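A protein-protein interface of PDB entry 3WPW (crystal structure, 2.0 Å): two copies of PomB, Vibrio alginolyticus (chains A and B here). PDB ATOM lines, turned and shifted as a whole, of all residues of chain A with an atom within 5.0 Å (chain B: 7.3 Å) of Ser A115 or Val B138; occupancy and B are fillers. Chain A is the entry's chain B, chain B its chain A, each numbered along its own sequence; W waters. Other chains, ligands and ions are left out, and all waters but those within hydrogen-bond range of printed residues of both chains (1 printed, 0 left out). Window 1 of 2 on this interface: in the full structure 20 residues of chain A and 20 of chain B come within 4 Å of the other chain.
Ser A115 touches just these residues of chain B: Val B119 and Val B138. Of chain A, only Trp A111, Ser A115, Arg A139 and Gly A140 come within 4 Å of Val B138. No residue of chain B comes within 4 Å of Ser A114. Printed residues of chain B within 4 Å of Gly A140: Val B138. Of the printed residues of chain A, Leu B136 touches Trp A111. Printed residues of chain B within 4 Å of Arg A139: Val B138 and Arg B139. Of the printed residues of chain A, Arg B108 touches Gln A116 (3.0 Å) and Val A119 (3.5 Å). Of the printed residues of chain B, Asp A112 touches Gln B116 (2.6 Å) and Val B119 (3.96 Å). Asn A110 touches none of the printed residues of chain B. The nearest printed residue of chain B that does not touch Ser A115 is Gln B116 (4.2 Å). The nearest residue of chain A that does not touch Val B138 is Val A138 (4.2 Å). The nearest printed residue of chain A that does not touch Gly B140 is Arg A139 (4.9 Å).
The backbone carbonyl oxygen of Gln A116 is in hydrogen-bond range of the guanidinium group of Arg B108, 3.0 Å away. NE2 of Gln B116 is in hydrogen-bond range of OD2 of Asp A112 (2.6 Å). The backbone NH of Gly A140 lies within hydrogen-bond range of the backbone carbonyl oxygen of Val B138. N of Gly B140 lies within hydrogen-bond range of O of Val A138.
Water W1 lies within hydrogen-bond range of the side-chain carboxylate (OD1) of Asp B112 (2.6 Å) and the side-chain amide oxygen (OE1) of Gln A116 (2.9 Å).
The backbone NH (N) of Arg B139 sits at hydrogen-bond distance from the backbone carbonyl oxygen (O) of Val B93 (2.9 Å). The backbone carbonyl oxygen (O) of Arg B139 lies within hydrogen-bond range of the backbone NH (N) of Gly B95 (3.0 Å). OG of Ser B120 is in hydrogen-bond range of O of Gln B116. O of Trp A111 sits at hydrogen-bond distance from OG of Ser A114, at 3.2 Å. The side-chain hydroxyl (OG) of Ser A115 lies within hydrogen-bond range of the backbone carbonyl oxygen (O) of Trp A111 (2.7 Å). OD2 of Asp A112 lies within hydrogen-bond range of NE2 of Gln A116, at 3.0 Å.
Asp A112 touches Gln B116, but with the chains exchanged Gln A116 does not touch Asp B112 (4.6 Å). Asp A112 touches Val B119, and with the chains exchanged Val A119 touches Asp B112. Ser A115 touches Val B138, and with the chains exchanged Val A138 touches Ser B115. Val A138 touches Arg B139, and with the chains exchanged Arg A139 touches Val B138. Of the 20 pairs that touch across the chains among the printed residues, 16 have their exchanged pair printed and touching as well.
Printed residues of chain B that touch a printed residue of chain A: Arg B108, Trp B111, Asp B112, Ser B115, Gln B116, Val B119, Leu B136, Val B138, Arg B139 and Gly B140. Hydrophobic or aromatic side chains of chain B that line the printed part of chain A: Trp B111, Val B119, Leu B136 and Val B138. Printed residues of chain A that touch a printed residue of chain B: Trp A111, Asp A112, Ser A115, Gln A116, Val A119, Val A138, Arg A139 and Gly A140. Hydrophobic or aromatic side chains of chain A within 4 Å of the printed part of chain B: Trp A111, Val A119 and Val A138.
Among the printed residues, pairs that only touch across the chains: Val A138 with Ser B115 (3.0 Å), Arg A139 with Val B138 (3.1 Å), Val A138 with Arg B139 (3.1 Å), Trp A111 with Leu B136 (3.2 Å), Ser A115 with Val B138 (3.3 Å), Ser A115 with Val B119 (3.4 Å), Val A119 with Arg B108 (3.5 Å), Gln A116 with Gln B116 (3.6 Å), Val A119 with Ser B115 (3.6 Å), Val A119 with Trp B111 (3.6 Å), Trp A111 with Val B119 (3.8 Å), Val A138 with Trp B111 (3.9 Å), Val A119 with Asp B112 (3.9 Å), Arg A139 with Arg B139 (3.9 Å), Trp A111 with Val B138 (3.9 Å) and Asp A112 with Val B119 (3.96 Å).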
ATOM      1  N   ASN A 110      38.381 -14.446 -25.437  1.00  0.00           N
ATOM      2  CA  ASN A 110      37.598 -14.101 -24.256  1.00  0.00           C
ATOM      3  C   ASN A 110      36.091 -13.999 -24.518  1.00  0.00           C
ATOM      4  O   ASN A 110      35.282 -14.261 -23.605  1.00  0.00           O
ATOM      5  CB  ASN A 110      38.121 -12.814 -23.614  1.00  0.00           C
ATOM      6  CG  ASN A 110      39.332 -13.055 -22.716  1.00  0.00           C
ATOM      7  OD1 ASN A 110      39.448 -14.102 -22.082  1.00  0.00           O
ATOM      8  ND2 ASN A 110      40.244 -12.078 -22.659  1.00  0.00           N
ATOM      9  N   TRP A 111      35.700 -13.642 -25.748  1.00  0.00           N
ATOM     10  CA  TRP A 111      34.288 -13.732 -26.132  1.00  0.00           C
ATOM     11  C   TRP A 111      33.796 -15.160 -25.988  1.00  0.00           C
ATOM     12  O   TRP A 111      32.706 -15.420 -25.453  1.00  0.00           O
ATOM     13  CB  TRP A 111      34.079 -13.299 -27.581  1.00  0.00           C
ATOM     14  CG  TRP A 111      34.435 -11.882 -27.803  1.00  0.00           C
ATOM     15  CD1 TRP A 111      35.418 -11.385 -28.631  1.00  0.00           C
ATOM     16  CD2 TRP A 111      33.830 -10.758 -27.174  1.00  0.00           C
ATOM     17  NE1 TRP A 111      35.435 -10.019 -28.555  1.00  0.00           N
ATOM     18  CE2 TRP A 111      34.474  -9.605 -27.671  1.00  0.00           C
ATOM     19  CE3 TRP A 111      32.800 -10.614 -26.238  1.00  0.00           C
ATOM     20  CZ2 TRP A 111      34.125  -8.318 -27.252  1.00  0.00           C
ATOM     21  CZ3 TRP A 111      32.449  -9.347 -25.825  1.00  0.00           C
ATOM     22  CH2 TRP A 111      33.117  -8.205 -26.331  1.00  0.00           C
ATOM     23  N   ASP A 112      34.597 -16.072 -26.523  1.00  0.00           N
ATOM     24  CA  ASP A 112      34.290 -17.488 -26.548  1.00  0.00           C
ATOM     25  C   ASP A 112      34.232 -18.025 -25.113  1.00  0.00           C
ATOM     26  O   ASP A 112      33.234 -18.614 -24.711  1.00  0.00           O
ATOM     27  CB  ASP A 112      35.361 -18.219 -27.372  1.00  0.00           C
ATOM     28  CG  ASP A 112      34.996 -19.668 -27.688  1.00  0.00           C
ATOM     29  OD1 ASP A 112      35.821 -20.376 -28.321  1.00  0.00           O
ATOM     30  OD2 ASP A 112      33.903 -20.109 -27.301  1.00  0.00           O
ATOM     31  N   LEU A 113      35.303 -17.830 -24.347  1.00  0.00           N
ATOM     32  CA  LEU A 113      35.325 -18.308 -22.957  1.00  0.00           C
ATOM     33  C   LEU A 113      34.155 -17.778 -22.130  1.00  0.00           C
ATOM     34  O   LEU A 113      33.497 -18.536 -21.421  1.00  0.00           O
ATOM     35  CB  LEU A 113      36.637 -17.933 -22.257  1.00  0.00           C
ATOM     36  CG  LEU A 113      36.722 -18.340 -20.778  1.00  0.00           C
ATOM     37  CD1 LEU A 113      36.405 -19.829 -20.594  1.00  0.00           C
ATOM     38  CD2 LEU A 113      38.118 -18.022 -20.220  1.00  0.00           C
ATOM     39  N   SER A 114      33.897 -16.477 -22.218  1.00  0.00           N
ATOM     40  CA  SER A 114      32.876 -15.871 -21.366  1.00  0.00           C
ATOM     41  C   SER A 114      31.472 -16.361 -21.754  1.00  0.00           C
ATOM     42  O   SER A 114      30.658 -16.698 -20.872  1.00  0.00           O
ATOM     43  CB  SER A 114      32.986 -14.338 -21.377  1.00  0.00           C
ATOM     44  OG  SER A 114      32.744 -13.800 -22.673  1.00  0.00           O
ATOM     45  N   SER A 115      31.214 -16.424 -23.067  1.00  0.00           N
ATOM     46  CA  SER A 115      30.006 -17.012 -23.635  1.00  0.00           C
ATOM     47  C   SER A 115      29.768 -18.435 -23.139  1.00  0.00           C
ATOM     48  O   SER A 115      28.671 -18.784 -22.702  1.00  0.00           O
ATOM     49  CB  SER A 115      30.123 -17.087 -25.184  1.00  0.00           C
ATOM     50  OG  SER A 115      30.070 -15.807 -25.765  1.00  0.00           O
ATOM     51  N   GLN A 116      30.783 -19.276 -23.260  1.00  0.00           N
ATOM     52  CA  GLN A 116      30.639 -20.696 -22.911  1.00  0.00           C
ATOM     53  C   GLN A 116      30.359 -20.901 -21.419  1.00  0.00           C
ATOM     54  O   GLN A 116      29.678 -21.850 -21.024  1.00  0.00           O
ATOM     55  CB  GLN A 116      31.871 -21.508 -23.347  1.00  0.00           C
ATOM     56  CG  GLN A 116      32.062 -21.609 -24.872  1.00  0.00           C
ATOM     57  CD  GLN A 116      32.611 -22.967 -25.318  1.00  0.00           C
ATOM     58  OE1 GLN A 116      32.176 -24.018 -24.835  1.00  0.00           O
ATOM     59  NE2 GLN A 116      33.571 -22.948 -26.245  1.00  0.00           N
ATOM     60  N   ARG A 117      30.897 -20.013 -20.589  1.00  0.00           N
ATOM     61  CA  ARG A 117      30.624 -20.063 -19.164  1.00  0.00           C
ATOM     62  C   ARG A 117      29.161 -19.776 -18.893  1.00  0.00           C
ATOM     63  O   ARG A 117      28.538 -20.428 -18.052  1.00  0.00           O
ATOM     64  CB  ARG A 117      31.514 -19.075 -18.404  1.00  0.00           C
ATOM     65  CG  ARG A 117      32.903 -19.609 -18.238  1.00  0.00           C
ATOM     66  CD  ARG A 117      33.738 -18.731 -17.312  1.00  0.00           C
ATOM     67  NE  ARG A 117      34.952 -19.442 -16.927  1.00  0.00           N
ATOM     68  CZ  ARG A 117      35.870 -18.963 -16.103  1.00  0.00           C
ATOM     69  NH1 ARG A 117      35.727 -17.741 -15.580  1.00  0.00           N
ATOM     70  NH2 ARG A 117      36.926 -19.704 -15.813  1.00  0.00           N
ATOM     71  N   ALA A 118      28.612 -18.804 -19.612  1.00  0.00           N
ATOM     72  CA  ALA A 118      27.196 -18.481 -19.496  1.00  0.00           C
ATOM     73  C   ALA A 118      26.362 -19.652 -19.973  1.00  0.00           C
ATOM     74  O   ALA A 118      25.363 -20.012 -19.346  1.00  0.00           O
ATOM     75  CB  ALA A 118      26.855 -17.225 -20.311  1.00  0.00           C
ATOM     76  N   VAL A 119      26.757 -20.223 -21.108  1.00  0.00           N
ATOM     77  CA  VAL A 119      26.070 -21.415 -21.632  1.00  0.00           C
ATOM     78  C   VAL A 119      26.055 -22.547 -20.586  1.00  0.00           C
ATOM     79  O   VAL A 119      25.013 -23.138 -20.322  1.00  0.00           O
ATOM     80  CB  VAL A 119      26.690 -21.909 -22.953  1.00  0.00           C
ATOM     81  CG1 VAL A 119      26.100 -23.285 -23.360  1.00  0.00           C
ATOM     82  CG2 VAL A 119      26.441 -20.891 -24.103  1.00  0.00           C
ATOM     83  N   VAL A 138      21.789 -15.824 -22.918  1.00  0.00           N
ATOM     84  CA  VAL A 138      23.190 -15.992 -22.544  1.00  0.00           C
ATOM     85  C   VAL A 138      24.009 -14.915 -23.207  1.00  0.00           C
ATOM     86  O   VAL A 138      23.774 -14.591 -24.363  1.00  0.00           O
ATOM     87  CB  VAL A 138      23.763 -17.411 -22.841  1.00  0.00           C
ATOM     88  CG1 VAL A 138      22.872 -18.505 -22.197  1.00  0.00           C
ATOM     89  CG2 VAL A 138      23.881 -17.658 -24.305  1.00  0.00           C
ATOM     90  N   ARG A 139      24.946 -14.347 -22.449  1.00  0.00           N
ATOM     91  CA  ARG A 139      25.825 -13.289 -22.947  1.00  0.00           C
ATOM     92  C   ARG A 139      27.270 -13.606 -22.605  1.00  0.00           C
ATOM     93  O   ARG A 139      27.551 -14.197 -21.554  1.00  0.00           O
ATOM     94  CB  ARG A 139      25.490 -11.943 -22.301  1.00  0.00           C
ATOM     95  CG  ARG A 139      24.130 -11.389 -22.591  1.00  0.00           C
ATOM     96  CD  ARG A 139      24.063  -9.885 -22.268  1.00  0.00           C
ATOM     97  NE  ARG A 139      24.539  -9.572 -20.920  1.00  0.00           N
ATOM     98  CZ  ARG A 139      24.600  -8.340 -20.423  1.00  0.00           C
ATOM     99  NH1 ARG A 139      24.205  -7.312 -21.163  1.00  0.00           N
ATOM    100  NH2 ARG A 139      25.045  -8.133 -19.192  1.00  0.00           N
ATOM    101  N   GLY A 140      28.179 -13.225 -23.498  1.00  0.00           N
ATOM    102  CA  GLY A 140      29.607 -13.274 -23.225  1.00  0.00           C
ATOM    103  C   GLY A 140      30.076 -11.826 -23.307  1.00  0.00           C
ATOM    104  O   GLY A 140      29.935 -11.180 -24.339  1.00  0.00           O
ATOM    105  N   VAL B  91      27.816  -2.380 -29.978  1.00  0.00           N
ATOM    106  CA  VAL B  91      27.478  -3.274 -31.081  1.00  0.00           C
ATOM    107  C   VAL B  91      27.143  -4.658 -30.477  1.00  0.00           C
ATOM    108  O   VAL B  91      28.005  -5.343 -29.931  1.00  0.00           O
ATOM    109  CB  VAL B  91      28.639  -3.335 -32.081  1.00  0.00           C
ATOM    110  CG1 VAL B  91      28.316  -4.250 -33.241  1.00  0.00           C
ATOM    111  CG2 VAL B  91      28.944  -1.911 -32.591  1.00  0.00           C
ATOM    112  N   ARG B  92      25.875  -5.040 -30.515  1.00  0.00           N
ATOM    113  CA  ARG B  92      25.479  -6.283 -29.853  1.00  0.00           C
ATOM    114  C   ARG B  92      25.259  -7.340 -30.925  1.00  0.00           C
ATOM    115  O   ARG B  92      24.388  -7.191 -31.774  1.00  0.00           O
ATOM    116  CB  ARG B  92      24.223  -6.054 -29.009  1.00  0.00           C
ATOM    117  CG  ARG B  92      23.794  -7.224 -28.153  1.00  0.00           C
ATOM    118  CD  ARG B  92      22.429  -6.926 -27.491  1.00  0.00           C
ATOM    119  NE  ARG B  92      21.382  -6.731 -28.499  1.00  0.00           N
ATOM    120  CZ  ARG B  92      20.155  -6.282 -28.244  1.00  0.00           C
ATOM    121  NH1 ARG B  92      19.796  -5.971 -27.004  1.00  0.00           N
ATOM    122  NH2 ARG B  92      19.286  -6.134 -29.235  1.00  0.00           N
ATOM    123  N   VAL B  93      26.076  -8.390 -30.893  1.00  0.00           N
ATOM    124  CA  VAL B  93      25.997  -9.457 -31.880  1.00  0.00           C
ATOM    125  C   VAL B  93      25.233 -10.636 -31.278  1.00  0.00           C
ATOM    126  O   VAL B  93      25.666 -11.211 -30.274  1.00  0.00           O
ATOM    127  CB  VAL B  93      27.402  -9.917 -32.291  1.00  0.00           C
ATOM    128  CG1 VAL B  93      27.329 -10.977 -33.362  1.00  0.00           C
ATOM    129  CG2 VAL B  93      28.257  -8.680 -32.792  1.00  0.00           C
ATOM    130  N   SER B  94      24.115 -10.999 -31.903  1.00  0.00           N
ATOM    131  CA  SER B  94      23.215 -11.986 -31.321  1.00  0.00           C
ATOM    132  C   SER B  94      22.974 -13.148 -32.273  1.00  0.00           C
ATOM    133  O   SER B  94      22.495 -12.948 -33.395  1.00  0.00           O
ATOM    134  CB  SER B  94      21.872 -11.343 -30.962  1.00  0.00           C
ATOM    135  OG  SER B  94      21.984 -10.296 -30.009  1.00  0.00           O
ATOM    136  N   GLY B  95      23.281 -14.358 -31.803  1.00  0.00           N
ATOM    137  CA  GLY B  95      22.983 -15.575 -32.533  1.00  0.00           C
ATOM    138  C   GLY B  95      21.645 -16.204 -32.181  1.00  0.00           C
ATOM    139  O   GLY B  95      21.232 -16.205 -31.005  1.00  0.00           O
ATOM    140  N   ARG B 108      26.693 -28.249 -27.258  1.00  0.00           N
ATOM    141  CA  ARG B 108      25.902 -28.852 -26.187  1.00  0.00           C
ATOM    142  C   ARG B 108      24.417 -28.522 -26.262  1.00  0.00           C
ATOM    143  O   ARG B 108      23.591 -29.234 -25.693  1.00  0.00           O
ATOM    144  CB  ARG B 108      26.447 -28.409 -24.829  1.00  0.00           C
ATOM    145  CG  ARG B 108      27.957 -28.457 -24.716  1.00  0.00           C
ATOM    146  CD  ARG B 108      28.396 -27.988 -23.324  1.00  0.00           C
ATOM    147  NE  ARG B 108      28.707 -26.562 -23.295  1.00  0.00           N
ATOM    148  CZ  ARG B 108      28.892 -25.867 -22.180  1.00  0.00           C
ATOM    149  NH1 ARG B 108      28.769 -26.474 -21.006  1.00  0.00           N
ATOM    150  NH2 ARG B 108      29.191 -24.569 -22.240  1.00  0.00           N
ATOM    151  N   TRP B 111      21.942 -22.935 -27.171  1.00  0.00           N
ATOM    152  CA  TRP B 111      22.617 -21.801 -26.506  1.00  0.00           C
ATOM    153  C   TRP B 111      24.071 -21.735 -26.934  1.00  0.00           C
ATOM    154  O   TRP B 111      24.644 -20.656 -27.200  1.00  0.00           O
ATOM    155  CB  TRP B 111      22.573 -21.936 -24.977  1.00  0.00           C
ATOM    156  CG  TRP B 111      21.188 -21.934 -24.383  1.00  0.00           C
ATOM    157  CD1 TRP B 111      20.569 -22.977 -23.725  1.00  0.00           C
ATOM    158  CD2 TRP B 111      20.257 -20.854 -24.383  1.00  0.00           C
ATOM    159  NE1 TRP B 111      19.309 -22.597 -23.322  1.00  0.00           N
ATOM    160  CE2 TRP B 111      19.092 -21.298 -23.710  1.00  0.00           C
ATOM    161  CE3 TRP B 111      20.285 -19.547 -24.880  1.00  0.00           C
ATOM    162  CZ2 TRP B 111      17.974 -20.486 -23.541  1.00  0.00           C
ATOM    163  CZ3 TRP B 111      19.165 -18.742 -24.708  1.00  0.00           C
ATOM    164  CH2 TRP B 111      18.028 -19.215 -24.050  1.00  0.00           C
ATOM    165  N   ASP B 112      24.678 -22.907 -26.962  1.00  0.00           N
ATOM    166  CA  ASP B 112      26.053 -23.074 -27.384  1.00  0.00           C
ATOM    167  C   ASP B 112      26.256 -22.658 -28.849  1.00  0.00           C
ATOM    168  O   ASP B 112      27.121 -21.842 -29.172  1.00  0.00           O
ATOM    169  CB  ASP B 112      26.446 -24.536 -27.208  1.00  0.00           C
ATOM    170  CG  ASP B 112      27.935 -24.733 -27.211  1.00  0.00           C
ATOM    171  OD1 ASP B 112      28.389 -25.780 -26.708  1.00  0.00           O
ATOM    172  OD2 ASP B 112      28.649 -23.833 -27.711  1.00  0.00           O
ATOM    173  N   SER B 114      24.197 -20.939 -30.881  1.00  0.00           N
ATOM    174  CA  SER B 114      23.829 -19.546 -31.154  1.00  0.00           C
ATOM    175  C   SER B 114      24.906 -18.587 -30.636  1.00  0.00           C
ATOM    176  O   SER B 114      25.282 -17.620 -31.309  1.00  0.00           O
ATOM    177  CB  SER B 114      22.428 -19.201 -30.620  1.00  0.00           C
ATOM    178  OG  SER B 114      22.324 -19.282 -29.197  1.00  0.00           O
ATOM    179  N   SER B 115      25.429 -18.884 -29.454  1.00  0.00           N
ATOM    180  CA  SER B 115      26.490 -18.096 -28.836  1.00  0.00           C
ATOM    181  C   SER B 115      27.748 -18.094 -29.689  1.00  0.00           C
ATOM    182  O   SER B 115      28.362 -17.052 -29.948  1.00  0.00           O
ATOM    183  CB  SER B 115      26.834 -18.697 -27.461  1.00  0.00           C
ATOM    184  OG  SER B 115      25.894 -18.284 -26.500  1.00  0.00           O
ATOM    185  N   GLN B 116      28.161 -19.279 -30.101  1.00  0.00           N
ATOM    186  CA  GLN B 116      29.389 -19.410 -30.886  1.00  0.00           C
ATOM    187  C   GLN B 116      29.339 -18.699 -32.220  1.00  0.00           C
ATOM    188  O   GLN B 116      30.356 -18.184 -32.680  1.00  0.00           O
ATOM    189  CB  GLN B 116      29.771 -20.882 -31.018  1.00  0.00           C
ATOM    190  CG  GLN B 116      30.338 -21.423 -29.717  1.00  0.00           C
ATOM    191  CD  GLN B 116      31.490 -20.567 -29.210  1.00  0.00           C
ATOM    192  OE1 GLN B 116      32.486 -20.381 -29.914  1.00  0.00           O
ATOM    193  NE2 GLN B 116      31.350 -20.015 -27.994  1.00  0.00           N
ATOM    194  N   ARG B 117      28.160 -18.647 -32.834  1.00  0.00           N
ATOM    195  CA  ARG B 117      28.001 -17.891 -34.069  1.00  0.00           C
ATOM    196  C   ARG B 117      28.190 -16.404 -33.821  1.00  0.00           C
ATOM    197  O   ARG B 117      28.898 -15.722 -34.568  1.00  0.00           O
ATOM    198  CB  ARG B 117      26.630 -18.166 -34.694  1.00  0.00           C
ATOM    199  CG  ARG B 117      26.557 -19.526 -35.343  1.00  0.00           C
ATOM    200  CD  ARG B 117      25.345 -19.670 -36.233  1.00  0.00           C
ATOM    201  NE  ARG B 117      25.457 -20.863 -37.062  1.00  0.00           N
ATOM    202  CZ  ARG B 117      24.471 -21.342 -37.817  1.00  0.00           C
ATOM    203  NH1 ARG B 117      23.289 -20.730 -37.845  1.00  0.00           N
ATOM    204  NH2 ARG B 117      24.672 -22.432 -38.539  1.00  0.00           N
ATOM    205  N   ALA B 118      27.575 -15.886 -32.766  1.00  0.00           N
ATOM    206  CA  ALA B 118      27.821 -14.487 -32.414  1.00  0.00           C
ATOM    207  C   ALA B 118      29.311 -14.261 -32.129  1.00  0.00           C
ATOM    208  O   ALA B 118      29.888 -13.242 -32.530  1.00  0.00           O
ATOM    209  CB  ALA B 118      26.959 -14.072 -31.221  1.00  0.00           C
ATOM    210  N   VAL B 119      29.940 -15.216 -31.451  1.00  0.00           N
ATOM    211  CA  VAL B 119      31.368 -15.111 -31.178  1.00  0.00           C
ATOM    212  C   VAL B 119      32.159 -14.969 -32.496  1.00  0.00           C
ATOM    213  O   VAL B 119      32.996 -14.086 -32.631  1.00  0.00           O
ATOM    214  CB  VAL B 119      31.905 -16.306 -30.344  1.00  0.00           C
ATOM    215  CG1 VAL B 119      33.440 -16.323 -30.347  1.00  0.00           C
ATOM    216  CG2 VAL B 119      31.376 -16.246 -28.925  1.00  0.00           C
ATOM    217  N   SER B 120      31.879 -15.824 -33.470  1.00  0.00           N
ATOM    218  CA  SER B 120      32.591 -15.756 -34.754  1.00  0.00           C
ATOM    219  C   SER B 120      32.484 -14.378 -35.400  1.00  0.00           C
ATOM    220  O   SER B 120      33.487 -13.811 -35.853  1.00  0.00           O
ATOM    221  CB  SER B 120      32.077 -16.817 -35.722  1.00  0.00           C
ATOM    222  OG  SER B 120      32.244 -18.103 -35.165  1.00  0.00           O
ATOM    223  N   VAL B 121      31.268 -13.842 -35.437  1.00  0.00           N
ATOM    224  CA  VAL B 121      31.032 -12.551 -36.066  1.00  0.00           C
ATOM    225  C   VAL B 121      31.767 -11.442 -35.295  1.00  0.00           C
ATOM    226  O   VAL B 121      32.408 -10.585 -35.898  1.00  0.00           O
ATOM    227  CB  VAL B 121      29.527 -12.262 -36.172  1.00  0.00           C
ATOM    228  CG1 VAL B 121      29.271 -10.835 -36.613  1.00  0.00           C
ATOM    229  CG2 VAL B 121      28.873 -13.255 -37.134  1.00  0.00           C
ATOM    230  N   ALA B 122      31.709 -11.473 -33.967  1.00  0.00           N
ATOM    231  CA  ALA B 122      32.380 -10.444 -33.153  1.00  0.00           C
ATOM    232  C   ALA B 122      33.889 -10.437 -33.382  1.00  0.00           C
ATOM    233  O   ALA B 122      34.516  -9.379 -33.524  1.00  0.00           O
ATOM    234  CB  ALA B 122      32.065 -10.647 -31.658  1.00  0.00           C
ATOM    235  N   GLN B 123      34.474 -11.627 -33.405  1.00  0.00           N
ATOM    236  CA  GLN B 123      35.914 -11.760 -33.599  1.00  0.00           C
ATOM    237  C   GLN B 123      36.303 -11.167 -34.948  1.00  0.00           C
ATOM    238  O   GLN B 123      37.329 -10.491 -35.062  1.00  0.00           O
ATOM    239  CB  GLN B 123      36.345 -13.230 -33.486  1.00  0.00           C
ATOM    240  CG  GLN B 123      36.349 -13.767 -32.030  1.00  0.00           C
ATOM    241  CD  GLN B 123      36.481 -15.275 -31.965  1.00  0.00           C
ATOM    242  OE1 GLN B 123      36.609 -15.860 -30.884  1.00  0.00           O
ATOM    243  NE2 GLN B 123      36.439 -15.918 -33.126  1.00  0.00           N
ATOM    244  N   LEU B 136      31.713  -4.211 -28.276  1.00  0.00           N
ATOM    245  CA  LEU B 136      31.034  -5.452 -28.642  1.00  0.00           C
ATOM    246  C   LEU B 136      30.330  -6.081 -27.440  1.00  0.00           C
ATOM    247  O   LEU B 136      30.794  -5.966 -26.315  1.00  0.00           O
ATOM    248  CB  LEU B 136      32.037  -6.457 -29.208  1.00  0.00           C
ATOM    249  CG  LEU B 136      32.428  -6.258 -30.672  1.00  0.00           C
ATOM    250  CD1 LEU B 136      33.706  -7.027 -31.032  1.00  0.00           C
ATOM    251  CD2 LEU B 136      31.263  -6.670 -31.566  1.00  0.00           C
ATOM    252  N   ARG B 137      29.216  -6.759 -27.698  1.00  0.00           N
ATOM    253  CA  ARG B 137      28.614  -7.636 -26.712  1.00  0.00           C
ATOM    254  C   ARG B 137      28.162  -8.863 -27.479  1.00  0.00           C
ATOM    255  O   ARG B 137      27.687  -8.738 -28.597  1.00  0.00           O
ATOM    256  CB  ARG B 137      27.409  -6.979 -26.014  1.00  0.00           C
ATOM    257  CG  ARG B 137      27.689  -5.651 -25.284  1.00  0.00           C
ATOM    258  CD  ARG B 137      28.635  -5.850 -24.114  1.00  0.00           C
ATOM    259  NE  ARG B 137      28.792  -4.643 -23.298  1.00  0.00           N
ATOM    260  CZ  ARG B 137      29.671  -3.682 -23.579  1.00  0.00           C
ATOM    261  NH1 ARG B 137      30.431  -3.801 -24.656  1.00  0.00           N
ATOM    262  NH2 ARG B 137      29.786  -2.610 -22.799  1.00  0.00           N
ATOM    263  N   VAL B 138      28.291 -10.045 -26.879  1.00  0.00           N
ATOM    264  CA  VAL B 138      27.917 -11.273 -27.573  1.00  0.00           C
ATOM    265  C   VAL B 138      26.757 -11.905 -26.823  1.00  0.00           C
ATOM    266  O   VAL B 138      26.769 -11.920 -25.605  1.00  0.00           O
ATOM    267  CB  VAL B 138      29.123 -12.248 -27.648  1.00  0.00           C
ATOM    268  CG1 VAL B 138      28.666 -13.666 -27.805  1.00  0.00           C
ATOM    269  CG2 VAL B 138      30.101 -11.845 -28.786  1.00  0.00           C
ATOM    270  N   ARG B 139      25.744 -12.368 -27.562  1.00  0.00           N
ATOM    271  CA  ARG B 139      24.587 -13.034 -26.969  1.00  0.00           C
ATOM    272  C   ARG B 139      24.251 -14.278 -27.775  1.00  0.00           C
ATOM    273  O   ARG B 139      24.317 -14.261 -29.012  1.00  0.00           O
ATOM    274  CB  ARG B 139      23.354 -12.137 -27.019  1.00  0.00           C
ATOM    275  CG  ARG B 139      23.496 -10.776 -26.391  1.00  0.00           C
ATOM    276  CD  ARG B 139      22.090 -10.239 -26.071  1.00  0.00           C
ATOM    277  NE  ARG B 139      21.331  -9.935 -27.289  1.00  0.00           N
ATOM    278  CZ  ARG B 139      20.021  -9.698 -27.326  1.00  0.00           C
ATOM    279  NH1 ARG B 139      19.297  -9.733 -26.213  1.00  0.00           N
ATOM    280  NH2 ARG B 139      19.429  -9.425 -28.480  1.00  0.00           N
ATOM    281  N   GLY B 140      23.869 -15.344 -27.072  1.00  0.00           N
ATOM    282  CA  GLY B 140      23.211 -16.478 -27.686  1.00  0.00           C
ATOM    283  C   GLY B 140      21.752 -16.469 -27.241  1.00  0.00           C
ATOM    284  O   GLY B 140      21.454 -16.460 -26.040  1.00  0.00           O
HETATM  285  O   HOH W   1      30.934 -26.202 -26.213  1.00  0.00           O
